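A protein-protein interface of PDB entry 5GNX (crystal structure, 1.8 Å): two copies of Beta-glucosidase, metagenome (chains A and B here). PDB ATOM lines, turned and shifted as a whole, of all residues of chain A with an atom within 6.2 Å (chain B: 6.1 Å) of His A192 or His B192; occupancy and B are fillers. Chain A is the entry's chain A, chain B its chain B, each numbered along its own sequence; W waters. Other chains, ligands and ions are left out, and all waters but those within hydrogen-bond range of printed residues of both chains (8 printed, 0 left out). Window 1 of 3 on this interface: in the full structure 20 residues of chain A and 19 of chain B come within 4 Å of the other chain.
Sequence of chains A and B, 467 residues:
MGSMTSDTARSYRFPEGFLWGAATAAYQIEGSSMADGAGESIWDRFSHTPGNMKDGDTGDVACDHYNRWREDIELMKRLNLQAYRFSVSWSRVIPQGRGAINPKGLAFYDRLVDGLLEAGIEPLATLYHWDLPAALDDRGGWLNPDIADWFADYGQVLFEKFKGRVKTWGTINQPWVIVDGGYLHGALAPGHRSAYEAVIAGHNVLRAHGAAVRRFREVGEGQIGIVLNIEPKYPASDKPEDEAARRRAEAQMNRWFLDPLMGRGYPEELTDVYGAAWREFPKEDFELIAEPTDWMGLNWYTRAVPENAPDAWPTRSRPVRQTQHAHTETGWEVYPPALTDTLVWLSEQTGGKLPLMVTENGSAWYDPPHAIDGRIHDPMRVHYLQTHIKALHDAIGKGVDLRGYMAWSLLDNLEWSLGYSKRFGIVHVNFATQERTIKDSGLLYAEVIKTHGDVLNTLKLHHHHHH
Among the printed residues, pairs that only touch across the chains: Asp A137 with Glu B197 (3.9 Å).
Printed residues of chain B within 4 Å of Asp A137: Glu B197 (3.9 Å).
Of the printed residues of chain B, Gly A140 touches Gly B140 (3.4 Å).
Gly A182 touches none of the printed residues of chain B.
His A192 touches just one residue of chain B: His B192 (3.3 Å).
Of the printed residues of chain A, Gly B140 touches Gly A140 (3.4 Å).
Of chain A, only His A192 comes within 4 Å of His B192.
Printed residues of chain A within 4 Å of Glu B197: Asp A137.
The nearest residue of chain A that does not touch His B192 is Glu A197 (4.8 Å).
The nearest printed residue of chain B that does not touch Gly A140 is Asp B137 (4.4 Å).
Printed residues of chain A that touch a printed residue of chain B: Asp A137, Gly A140 and His A192.
Among the printed residues, 3 pairs touch across the chains.
Among the printed residues, no Asp or Glu carboxylate lies within 4 Å of a Lys or Arg side-chain nitrogen of the other chain.
Water W4 lies within hydrogen-bond range of the side-chain carboxylate (OD2) of Asp B137 (2.6 Å), the side-chain carboxylate (OE2) of Glu A197 (2.7 Å) and a ring nitrogen (NE2) of His B192 (2.9 Å).
Water W8 lies within hydrogen-bond range of the side-chain carboxylate (OD2) of Asp A137 (2.6 Å), the side-chain carboxylate (OE2) of Glu B197 (2.7 Å) and a ring nitrogen (NE2) of His A192 (2.8 Å).
Water W3 bridges the side-chain carboxylate of Glu A197 (2.6 Å) and the backbone carbonyl oxygen of Pro B190 (2.7 Å).
Water W7 lies within hydrogen-bond range of the side-chain carboxylate of Asp B137 (2.7 Å) and the side-chain carboxylate of Glu A197 (3.0 Å).
Water W2 lies within hydrogen-bond range of N of Arg A193 and O of Gly B191.
Water W6 bridges the backbone NH of Arg B193 (2.9 Å) and the backbone carbonyl oxygen of Gly A191 (3.0 Å).
The backbone NH of Gly B140 sits close to the backbone NH of Gly A140.
A ring nitrogen (NE2) of His A192 lies close to a ring nitrogen (NE2) of His B192 (3.4 Å).
Asp A137 touches Glu B197, but with the chains exchanged Glu A197 does not touch Asp B137 (4.05 Å).
Gly A140 touches its own counterpart, Gly B140.
His A192 touches its own counterpart, His B192.
Positions printed for both chains: 137, 140, 143, 179, 180, 181, 182, 183, 184, 185, 186, 187, 188, 189, 190, 191, 192, 193, 194 and 197.
OE1 of Glu A197 is in hydrogen-bond range of ND1 of His A192.
The backbone NH of His A192 lies within hydrogen-bond range of the backbone carbonyl oxygen of Gly A182 (2.9 Å).
The backbone NH of Gly A186 sits at hydrogen-bond distance from the backbone carbonyl oxygen of His A192 (2.9 Å).
OG of Ser B194 is in hydrogen-bond range of N of Glu B197 (3.1 Å).
The backbone NH of Gly B186 sits at hydrogen-bond distance from the backbone carbonyl oxygen of His B192.
OE1 of Glu B197 sits at hydrogen-bond distance from ND1 of His B192 (2.5 Å).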
ATOM      1  N   ASP A 137      23.335 -16.711   0.395  1.00  0.00           N
ATOM      2  CA  ASP A 137      23.738 -16.861   1.789  1.00  0.00           C
ATOM      3  C   ASP A 137      22.516 -17.012   2.702  1.00  0.00           C
ATOM      4  O   ASP A 137      22.539 -17.794   3.698  1.00  0.00           O
ATOM      5  CB  ASP A 137      24.585 -15.679   2.219  1.00  0.00           C
ATOM      6  CG  ASP A 137      25.470 -16.013   3.441  1.00  0.00           C
ATOM      7  OD1 ASP A 137      26.214 -17.042   3.411  1.00  0.00           O
ATOM      8  OD2 ASP A 137      25.425 -15.260   4.397  1.00  0.00           O
ATOM      9  N   GLY A 140      21.622 -20.475   2.955  1.00  0.00           N
ATOM     10  CA  GLY A 140      22.631 -21.357   3.527  1.00  0.00           C
ATOM     11  C   GLY A 140      24.009 -21.234   2.906  1.00  0.00           C
ATOM     12  O   GLY A 140      24.965 -21.807   3.401  1.00  0.00           O
ATOM     13  N   LEU A 143      26.828 -23.943   2.746  1.00  0.00           N
ATOM     14  CA  LEU A 143      26.321 -25.056   3.508  1.00  0.00           C
ATOM     15  C   LEU A 143      25.171 -25.808   2.840  1.00  0.00           C
ATOM     16  O   LEU A 143      24.804 -26.903   3.274  1.00  0.00           O
ATOM     17  CB  LEU A 143      25.856 -24.606   4.885  1.00  0.00           C
ATOM     18  CG  LEU A 143      26.887 -23.803   5.671  1.00  0.00           C
ATOM     19  CD1 LEU A 143      26.289 -23.416   7.011  1.00  0.00           C
ATOM     20  CD2 LEU A 143      28.120 -24.657   5.821  1.00  0.00           C
ATOM     21  N   VAL A 179      36.818 -21.152   2.850  1.00  0.00           N
ATOM     22  CA  VAL A 179      36.289 -21.957   3.950  1.00  0.00           C
ATOM     23  C   VAL A 179      36.997 -21.700   5.269  1.00  0.00           C
ATOM     24  O   VAL A 179      36.346 -21.524   6.326  1.00  0.00           O
ATOM     25  CB  VAL A 179      36.365 -23.455   3.573  1.00  0.00           C
ATOM     26  CG1 VAL A 179      35.758 -24.288   4.692  1.00  0.00           C
ATOM     27  CG2 VAL A 179      35.547 -23.694   2.303  1.00  0.00           C
ATOM     28  N   ASP A 180      38.327 -21.686   5.241  1.00  0.00           N
ATOM     29  CA  ASP A 180      39.076 -21.425   6.476  1.00  0.00           C
ATOM     30  C   ASP A 180      38.775 -20.023   7.028  1.00  0.00           C
ATOM     31  O   ASP A 180      38.535 -19.853   8.221  1.00  0.00           O
ATOM     32  CB  ASP A 180      40.583 -21.622   6.225  1.00  0.00           C
ATOM     33  CG  ASP A 180      41.397 -21.558   7.491  1.00  0.00           C
ATOM     34  OD1 ASP A 180      41.790 -20.428   7.891  1.00  0.00           O
ATOM     35  OD2 ASP A 180      41.682 -22.644   8.085  1.00  0.00           O
ATOM     36  N   GLY A 181      38.751 -19.020   6.152  1.00  0.00           N
ATOM     37  CA  GLY A 181      38.435 -17.690   6.553  1.00  0.00           C
ATOM     38  C   GLY A 181      36.983 -17.386   6.775  1.00  0.00           C
ATOM     39  O   GLY A 181      36.642 -16.675   7.721  1.00  0.00           O
ATOM     40  N   GLY A 182      36.105 -17.896   5.909  1.00  0.00           N
ATOM     41  CA  GLY A 182      34.683 -17.547   5.930  1.00  0.00           C
ATOM     42  C   GLY A 182      33.835 -18.386   6.880  1.00  0.00           C
ATOM     43  O   GLY A 182      32.805 -17.904   7.341  1.00  0.00           O
ATOM     44  N   TYR A 183      34.232 -19.638   7.127  1.00  0.00           N
ATOM     45  CA  TYR A 183      33.430 -20.582   7.915  1.00  0.00           C
ATOM     46  C   TYR A 183      34.101 -21.169   9.140  1.00  0.00           C
ATOM     47  O   TYR A 183      33.430 -21.466  10.134  1.00  0.00           O
ATOM     48  CB  TYR A 183      32.910 -21.735   7.023  1.00  0.00           C
ATOM     49  CG  TYR A 183      31.871 -21.280   6.040  1.00  0.00           C
ATOM     50  CD1 TYR A 183      32.230 -20.771   4.783  1.00  0.00           C
ATOM     51  CD2 TYR A 183      30.492 -21.322   6.349  1.00  0.00           C
ATOM     52  CE1 TYR A 183      31.268 -20.324   3.878  1.00  0.00           C
ATOM     53  CE2 TYR A 183      29.518 -20.879   5.443  1.00  0.00           C
ATOM     54  CZ  TYR A 183      29.903 -20.388   4.211  1.00  0.00           C
ATOM     55  OH  TYR A 183      28.979 -19.942   3.309  1.00  0.00           O
ATOM     56  N   LEU A 184      35.421 -21.365   9.077  1.00  0.00           N
ATOM     57  CA  LEU A 184      36.124 -21.963  10.199  1.00  0.00           C
ATOM     58  C   LEU A 184      36.467 -20.925  11.251  1.00  0.00           C
ATOM     59  O   LEU A 184      36.202 -21.126  12.468  1.00  0.00           O
ATOM     60  CB  LEU A 184      37.416 -22.692   9.720  1.00  0.00           C
ATOM     61  CG  LEU A 184      38.221 -23.373  10.809  1.00  0.00           C
ATOM     62  CD1 LEU A 184      37.375 -24.430  11.553  1.00  0.00           C
ATOM     63  CD2 LEU A 184      39.426 -24.061  10.204  1.00  0.00           C
ATOM     64  N   HIS A 185      37.086 -19.841  10.821  1.00  0.00           N
ATOM     65  CA  HIS A 185      37.541 -18.814  11.745  1.00  0.00           C
ATOM     66  C   HIS A 185      36.745 -17.518  11.750  1.00  0.00           C
ATOM     67  O   HIS A 185      36.871 -16.723  12.686  1.00  0.00           O
ATOM     68  CB  HIS A 185      39.023 -18.521  11.544  1.00  0.00           C
ATOM     69  CG  HIS A 185      39.904 -19.679  11.857  1.00  0.00           C
ATOM     70  ND1 HIS A 185      40.040 -20.184  13.129  1.00  0.00           N
ATOM     71  CD2 HIS A 185      40.651 -20.481  11.057  1.00  0.00           C
ATOM     72  CE1 HIS A 185      40.851 -21.225  13.112  1.00  0.00           C
ATOM     73  NE2 HIS A 185      41.260 -21.418  11.864  1.00  0.00           N
ATOM     74  N   GLY A 186      35.959 -17.290  10.714  1.00  0.00           N
ATOM     75  CA  GLY A 186      35.124 -16.094  10.630  1.00  0.00           C
ATOM     76  C   GLY A 186      35.763 -14.774  10.324  1.00  0.00           C
ATOM     77  O   GLY A 186      35.101 -13.740  10.510  1.00  0.00           O
ATOM     78  N   ALA A 187      37.017 -14.737   9.863  1.00  0.00           N
ATOM     79  CA  ALA A 187      37.694 -13.486   9.641  1.00  0.00           C
ATOM     80  C   ALA A 187      37.316 -12.840   8.300  1.00  0.00           C
ATOM     81  O   ALA A 187      37.526 -11.657   8.090  1.00  0.00           O
ATOM     82  CB  ALA A 187      39.230 -13.672   9.696  1.00  0.00           C
ATOM     83  N   LEU A 188      36.697 -13.633   7.436  1.00  0.00           N
ATOM     84  CA  LEU A 188      36.229 -13.207   6.132  1.00  0.00           C
ATOM     85  C   LEU A 188      34.712 -13.499   6.027  1.00  0.00           C
ATOM     86  O   LEU A 188      34.184 -14.324   6.759  1.00  0.00           O
ATOM     87  CB  LEU A 188      36.952 -13.993   5.026  1.00  0.00           C
ATOM     88  CG  LEU A 188      38.482 -13.911   4.995  1.00  0.00           C
ATOM     89  CD1 LEU A 188      39.018 -14.747   3.824  1.00  0.00           C
ATOM     90  CD2 LEU A 188      38.903 -12.462   4.867  1.00  0.00           C
ATOM     91  N   ALA A 189      34.050 -12.803   5.117  1.00  0.00           N
ATOM     92  CA  ALA A 189      32.640 -13.089   4.812  1.00  0.00           C
ATOM     93  C   ALA A 189      32.433 -14.557   4.467  1.00  0.00           C
ATOM     94  O   ALA A 189      33.253 -15.169   3.747  1.00  0.00           O
ATOM     95  CB  ALA A 189      32.117 -12.195   3.687  1.00  0.00           C
ATOM     96  N   PRO A 190      31.359 -15.167   4.967  1.00  0.00           N
ATOM     97  CA  PRO A 190      30.225 -14.563   5.695  1.00  0.00           C
ATOM     98  C   PRO A 190      30.395 -14.519   7.196  1.00  0.00           C
ATOM     99  O   PRO A 190      29.385 -14.315   7.905  1.00  0.00           O
ATOM    100  CB  PRO A 190      29.052 -15.463   5.285  1.00  0.00           C
ATOM    101  CG  PRO A 190      29.714 -16.843   5.265  1.00  0.00           C
ATOM    102  CD  PRO A 190      31.108 -16.575   4.624  1.00  0.00           C
ATOM    103  N   GLY A 191      31.621 -14.723   7.709  1.00  0.00           N
ATOM    104  CA  GLY A 191      31.889 -14.543   9.135  1.00  0.00           C
ATOM    105  C   GLY A 191      31.373 -15.607  10.083  1.00  0.00           C
ATOM    106  O   GLY A 191      30.975 -15.280  11.202  1.00  0.00           O
ATOM    107  N   HIS A 192      31.349 -16.856   9.655  1.00  0.00           N
ATOM    108  CA  HIS A 192      31.001 -17.947  10.567  1.00  0.00           C
ATOM    109  C   HIS A 192      32.241 -18.525  11.200  1.00  0.00           C
ATOM    110  O   HIS A 192      33.328 -18.503  10.620  1.00  0.00           O
ATOM    111  CB  HIS A 192      30.216 -19.048   9.859  1.00  0.00           C
ATOM    112  CG  HIS A 192      28.946 -18.600   9.202  1.00  0.00           C
ATOM    113  ND1 HIS A 192      27.991 -19.490   8.777  1.00  0.00           N
ATOM    114  CD2 HIS A 192      28.479 -17.366   8.880  1.00  0.00           C
ATOM    115  CE1 HIS A 192      27.001 -18.832   8.194  1.00  0.00           C
ATOM    116  NE2 HIS A 192      27.282 -17.544   8.239  1.00  0.00           N
ATOM    117  N   ARG A 193      32.090 -19.087  12.405  1.00  0.00           N
ATOM    118  CA  ARG A 193      33.182 -19.738  13.083  1.00  0.00           C
ATOM    119  C   ARG A 193      32.727 -21.110  13.628  1.00  0.00           C
ATOM    120  O   ARG A 193      32.107 -21.213  14.710  1.00  0.00           O
ATOM    121  CB  ARG A 193      33.760 -18.807  14.195  1.00  0.00           C
ATOM    122  CG  ARG A 193      34.850 -19.460  15.043  1.00  0.00           C
ATOM    123  CD  ARG A 193      35.664 -18.466  15.890  1.00  0.00           C
ATOM    124  NE  ARG A 193      36.696 -19.125  16.658  1.00  0.00           N
ATOM    125  CZ  ARG A 193      36.479 -19.747  17.828  1.00  0.00           C
ATOM    126  NH1 ARG A 193      35.250 -19.756  18.344  1.00  0.00           N
ATOM    127  NH2 ARG A 193      37.466 -20.340  18.485  1.00  0.00           N
ATOM    128  N   SER A 194      32.969 -22.159  12.869  1.00  0.00           N
ATOM    129  CA  SER A 194      32.470 -23.498  13.183  1.00  0.00           C
ATOM    130  C   SER A 194      33.244 -24.579  12.399  1.00  0.00           C
ATOM    131  O   SER A 194      33.275 -24.522  11.160  1.00  0.00           O
ATOM    132  CB  SER A 194      30.993 -23.583  12.840  1.00  0.00           C
ATOM    133  OG  SER A 194      30.501 -24.892  12.902  1.00  0.00           O
ATOM    134  N   GLU A 197      30.591 -26.456  10.234  1.00  0.00           N
ATOM    135  CA  GLU A 197      30.278 -25.791   9.016  1.00  0.00           C
ATOM    136  C   GLU A 197      31.440 -25.833   8.061  1.00  0.00           C
ATOM    137  O   GLU A 197      31.227 -25.951   6.871  1.00  0.00           O
ATOM    138  CB  GLU A 197      29.884 -24.339   9.283  1.00  0.00           C
ATOM    139  CG  GLU A 197      28.602 -24.188  10.074  1.00  0.00           C
ATOM    140  CD  GLU A 197      28.153 -22.730  10.100  1.00  0.00           C
ATOM    141  OE1 GLU A 197      28.609 -21.944   9.246  1.00  0.00           O
ATOM    142  OE2 GLU A 197      27.344 -22.368  10.967  1.00  0.00           O
ATOM    143  N   ASP B 137      19.552 -24.928   9.347  1.00  0.00           N
ATOM    144  CA  ASP B 137      20.564 -23.880   9.390  1.00  0.00           C
ATOM    145  C   ASP B 137      21.449 -23.916   8.149  1.00  0.00           C
ATOM    146  O   ASP B 137      21.844 -22.862   7.635  1.00  0.00           O
ATOM    147  CB  ASP B 137      21.448 -24.000  10.617  1.00  0.00           C
ATOM    148  CG  ASP B 137      22.126 -22.679  10.953  1.00  0.00           C
ATOM    149  OD1 ASP B 137      21.417 -21.629  10.963  1.00  0.00           O
ATOM    150  OD2 ASP B 137      23.316 -22.693  11.188  1.00  0.00           O
ATOM    151  N   GLY B 140      19.977 -21.981   5.532  1.00  0.00           N
ATOM    152  CA  GLY B 140      19.840 -20.571   5.829  1.00  0.00           C
ATOM    153  C   GLY B 140      19.155 -20.225   7.127  1.00  0.00           C
ATOM    154  O   GLY B 140      19.157 -19.057   7.553  1.00  0.00           O
ATOM    155  N   LEU B 143      17.090 -17.131   8.074  1.00  0.00           N
ATOM    156  CA  LEU B 143      17.249 -16.220   6.938  1.00  0.00           C
ATOM    157  C   LEU B 143      16.469 -16.647   5.685  1.00  0.00           C
ATOM    158  O   LEU B 143      16.293 -15.846   4.751  1.00  0.00           O
ATOM    159  CB  LEU B 143      18.707 -16.054   6.596  1.00  0.00           C
ATOM    160  CG  LEU B 143      19.646 -15.616   7.737  1.00  0.00           C
ATOM    161  CD1 LEU B 143      21.031 -15.477   7.186  1.00  0.00           C
ATOM    162  CD2 LEU B 143      19.168 -14.311   8.387  1.00  0.00           C
ATOM    163  N   VAL B 179      17.120 -13.618  17.908  1.00  0.00           N
ATOM    164  CA  VAL B 179      17.649 -12.791  16.796  1.00  0.00           C
ATOM    165  C   VAL B 179      18.767 -11.901  17.318  1.00  0.00           C
ATOM    166  O   VAL B 179      19.871 -11.838  16.705  1.00  0.00           O
ATOM    167  CB  VAL B 179      16.514 -11.961  16.186  1.00  0.00           C
ATOM    168  CG1 VAL B 179      17.050 -11.043  15.105  1.00  0.00           C
ATOM    169  CG2 VAL B 179      15.482 -12.921  15.581  1.00  0.00           C
ATOM    170  N   ASP B 180      18.539 -11.210  18.418  1.00  0.00           N
ATOM    171  CA  ASP B 180      19.605 -10.339  18.959  1.00  0.00           C
ATOM    172  C   ASP B 180      20.856 -11.147  19.322  1.00  0.00           C
ATOM    173  O   ASP B 180      21.998 -10.726  19.047  1.00  0.00           O
ATOM    174  CB  ASP B 180      19.088  -9.543  20.191  1.00  0.00           C
ATOM    175  CG  ASP B 180      20.061  -8.457  20.628  1.00  0.00           C
ATOM    176  OD1 ASP B 180      20.990  -8.774  21.403  1.00  0.00           O
ATOM    177  OD2 ASP B 180      19.879  -7.315  20.242  1.00  0.00           O
ATOM    178  N   GLY B 181      20.662 -12.293  19.967  1.00  0.00           N
ATOM    179  CA  GLY B 181      21.780 -13.114  20.379  1.00  0.00           C
ATOM    180  C   GLY B 181      22.368 -13.969  19.251  1.00  0.00           C
ATOM    181  O   GLY B 181      23.581 -14.170  19.168  1.00  0.00           O
ATOM    182  N   GLY B 182      21.503 -14.516  18.411  1.00  0.00           N
ATOM    183  CA  GLY B 182      21.951 -15.467  17.404  1.00  0.00           C
ATOM    184  C   GLY B 182      22.410 -14.871  16.068  1.00  0.00           C
ATOM    185  O   GLY B 182      23.227 -15.482  15.381  1.00  0.00           O
ATOM    186  N   TYR B 183      21.881 -13.695  15.715  1.00  0.00           N
ATOM    187  CA  TYR B 183      22.128 -13.087  14.426  1.00  0.00           C
ATOM    188  C   TYR B 183      22.744 -11.702  14.490  1.00  0.00           C
ATOM    189  O   TYR B 183      23.500 -11.319  13.584  1.00  0.00           O
ATOM    190  CB  TYR B 183      20.842 -13.069  13.549  1.00  0.00           C
ATOM    191  CG  TYR B 183      20.432 -14.414  13.095  1.00  0.00           C
ATOM    192  CD1 TYR B 183      19.617 -15.235  13.893  1.00  0.00           C
ATOM    193  CD2 TYR B 183      20.930 -14.968  11.894  1.00  0.00           C
ATOM    194  CE1 TYR B 183      19.289 -16.526  13.481  1.00  0.00           C
ATOM    195  CE2 TYR B 183      20.578 -16.240  11.486  1.00  0.00           C
ATOM    196  CZ  TYR B 183      19.770 -17.023  12.287  1.00  0.00           C
ATOM    197  OH  TYR B 183      19.429 -18.281  11.870  1.00  0.00           O
ATOM    198  N   LEU B 184      22.393 -10.914  15.494  1.00  0.00           N
ATOM    199  CA  LEU B 184      22.886  -9.526  15.552  1.00  0.00           C
ATOM    200  C   LEU B 184      24.268  -9.465  16.205  1.00  0.00           C
ATOM    201  O   LEU B 184      25.187  -8.900  15.645  1.00  0.00           O
ATOM    202  CB  LEU B 184      21.914  -8.607  16.314  1.00  0.00           C
ATOM    203  CG  LEU B 184      22.339  -7.147  16.474  1.00  0.00           C
ATOM    204  CD1 LEU B 184      22.528  -6.517  15.084  1.00  0.00           C
ATOM    205  CD2 LEU B 184      21.284  -6.416  17.279  1.00  0.00           C
ATOM    206  N   HIS B 185      24.428 -10.077  17.385  1.00  0.00           N
ATOM    207  CA  HIS B 185      25.695 -10.013  18.115  1.00  0.00           C
ATOM    208  C   HIS B 185      26.490 -11.324  18.120  1.00  0.00           C
ATOM    209  O   HIS B 185      27.671 -11.331  18.434  1.00  0.00           O
ATOM    210  CB  HIS B 185      25.424  -9.563  19.551  1.00  0.00           C
ATOM    211  CG  HIS B 185      24.875  -8.160  19.627  1.00  0.00           C
ATOM    212  ND1 HIS B 185      25.613  -7.054  19.249  1.00  0.00           N
ATOM    213  CD2 HIS B 185      23.645  -7.705  19.933  1.00  0.00           C
ATOM    214  CE1 HIS B 185      24.875  -5.967  19.398  1.00  0.00           C
ATOM    215  NE2 HIS B 185      23.666  -6.340  19.810  1.00  0.00           N
ATOM    216  N   GLY B 186      25.815 -12.423  17.857  1.00  0.00           N
ATOM    217  CA  GLY B 186      26.483 -13.702  17.745  1.00  0.00           C
ATOM    218  C   GLY B 186      26.930 -14.376  19.033  1.00  0.00           C
ATOM    219  O   GLY B 186      27.712 -15.330  18.994  1.00  0.00           O
ATOM    220  N   ALA B 187      26.341 -14.002  20.155  1.00  0.00           N
ATOM    221  CA  ALA B 187      26.680 -14.629  21.429  1.00  0.00           C
ATOM    222  C   ALA B 187      25.998 -15.974  21.646  1.00  0.00           C
ATOM    223  O   ALA B 187      26.419 -16.754  22.497  1.00  0.00           O
ATOM    224  CB  ALA B 187      26.328 -13.722  22.583  1.00  0.00           C
ATOM    225  N   LEU B 188      24.982 -16.253  20.859  1.00  0.00           N
ATOM    226  CA  LEU B 188      24.188 -17.486  20.915  1.00  0.00           C
ATOM    227  C   LEU B 188      24.163 -18.158  19.540  1.00  0.00           C
ATOM    228  O   LEU B 188      24.432 -17.502  18.534  1.00  0.00           O
ATOM    229  CB  LEU B 188      22.740 -17.199  21.333  1.00  0.00           C
ATOM    230  CG  LEU B 188      22.552 -16.458  22.670  1.00  0.00           C
ATOM    231  CD1 LEU B 188      21.062 -16.143  22.951  1.00  0.00           C
ATOM    232  CD2 LEU B 188      23.118 -17.269  23.761  1.00  0.00           C
ATOM    233  N   ALA B 189      23.899 -19.451  19.496  1.00  0.00           N
ATOM    234  CA  ALA B 189      23.726 -20.129  18.224  1.00  0.00           C
ATOM    235  C   ALA B 189      22.686 -19.435  17.338  1.00  0.00           C
ATOM    236  O   ALA B 189      21.645 -18.972  17.836  1.00  0.00           O
ATOM    237  CB  ALA B 189      23.363 -21.595  18.431  1.00  0.00           C
ATOM    238  N   PRO B 190      22.935 -19.346  16.013  1.00  0.00           N
ATOM    239  CA  PRO B 190      24.066 -19.944  15.252  1.00  0.00           C
ATOM    240  C   PRO B 190      25.316 -19.069  15.191  1.00  0.00           C
ATOM    241  O   PRO B 190      26.203 -19.345  14.373  1.00  0.00           O
ATOM    242  CB  PRO B 190      23.463 -20.115  13.858  1.00  0.00           C
ATOM    243  CG  PRO B 190      22.611 -18.878  13.748  1.00  0.00           C
ATOM    244  CD  PRO B 190      21.933 -18.757  15.104  1.00  0.00           C
ATOM    245  N   GLY B 191      25.370 -17.980  15.957  1.00  0.00           N
ATOM    246  CA  GLY B 191      26.613 -17.243  16.163  1.00  0.00           C
ATOM    247  C   GLY B 191      26.964 -16.331  14.994  1.00  0.00           C
ATOM    248  O   GLY B 191      28.149 -16.186  14.658  1.00  0.00           O
ATOM    249  N   HIS B 192      25.955 -15.737  14.368  1.00  0.00           N
ATOM    250  CA  HIS B 192      26.153 -14.720  13.343  1.00  0.00           C
ATOM    251  C   HIS B 192      26.153 -13.326  13.953  1.00  0.00           C
ATOM    252  O   HIS B 192      25.526 -13.102  15.000  1.00  0.00           O
ATOM    253  CB  HIS B 192      25.080 -14.785  12.272  1.00  0.00           C
ATOM    254  CG  HIS B 192      24.992 -16.075  11.529  1.00  0.00           C
ATOM    255  ND1 HIS B 192      24.301 -16.173  10.354  1.00  0.00           N
ATOM    256  CD2 HIS B 192      25.469 -17.309  11.798  1.00  0.00           C
ATOM    257  CE1 HIS B 192      24.362 -17.424   9.915  1.00  0.00           C
ATOM    258  NE2 HIS B 192      25.053 -18.134  10.783  1.00  0.00           N
ATOM    259  N   ARG B 193      26.865 -12.375  13.308  1.00  0.00           N
ATOM    260  CA  ARG B 193      26.893 -11.004  13.754  1.00  0.00           C
ATOM    261  C   ARG B 193      26.676 -10.082  12.564  1.00  0.00           C
ATOM    262  O   ARG B 193      27.617  -9.748  11.806  1.00  0.00           O
ATOM    263  CB  ARG B 193      28.233 -10.679  14.455  1.00  0.00           C
ATOM    264  CG  ARG B 193      28.406  -9.242  14.875  1.00  0.00           C
ATOM    265  CD  ARG B 193      29.558  -9.091  15.881  1.00  0.00           C
ATOM    266  NE  ARG B 193      29.682  -7.700  16.329  1.00  0.00           N
ATOM    267  CZ  ARG B 193      30.332  -6.758  15.656  1.00  0.00           C
ATOM    268  NH1 ARG B 193      30.902  -7.087  14.511  1.00  0.00           N
ATOM    269  NH2 ARG B 193      30.433  -5.523  16.118  1.00  0.00           N
ATOM    270  N   SER B 194      25.453  -9.685  12.362  1.00  0.00           N
ATOM    271  CA  SER B 194      25.112  -8.891  11.182  1.00  0.00           C
ATOM    272  C   SER B 194      23.782  -8.196  11.417  1.00  0.00           C
ATOM    273  O   SER B 194      22.801  -8.880  11.693  1.00  0.00           O
ATOM    274  CB  SER B 194      25.017  -9.818   9.971  1.00  0.00           C
ATOM    275  OG  SER B 194      24.482  -9.141   8.831  1.00  0.00           O
ATOM    276  N   GLU B 197      21.402  -9.462   8.586  1.00  0.00           N
ATOM    277  CA  GLU B 197      20.774 -10.709   8.899  1.00  0.00           C
ATOM    278  C   GLU B 197      19.737 -10.607   9.996  1.00  0.00           C
ATOM    279  O   GLU B 197      18.696 -11.277   9.928  1.00  0.00           O
ATOM    280  CB  GLU B 197      21.809 -11.745   9.305  1.00  0.00           C
ATOM    281  CG  GLU B 197      22.760 -12.124   8.160  1.00  0.00           C
ATOM    282  CD  GLU B 197      23.687 -13.268   8.523  1.00  0.00           C
ATOM    283  OE1 GLU B 197      23.375 -14.035   9.476  1.00  0.00           O
ATOM    284  OE2 GLU B 197      24.717 -13.446   7.812  1.00  0.00           O
HETATM  285  O   HOH W   1      25.480 -12.713   5.063  1.00  0.00           O
HETATM  286  O   HOH W   2      29.543 -18.606  13.600  1.00  0.00           O
HETATM  287  O   HOH W   3      27.924 -20.821  13.000  1.00  0.00           O
HETATM  288  O   HOH W   4      25.112 -20.993  10.411  1.00  0.00           O
HETATM  289  O   HOH W   5      27.172 -13.142   8.825  1.00  0.00           O
HETATM  290  O   HOH W   6      28.561 -13.464  11.242  1.00  0.00           O
HETATM  291  O   HOH W   7      25.312 -23.959  12.585  1.00  0.00           O
HETATM  292  O   HOH W   8      25.498 -15.909   6.910  1.00  0.00           O
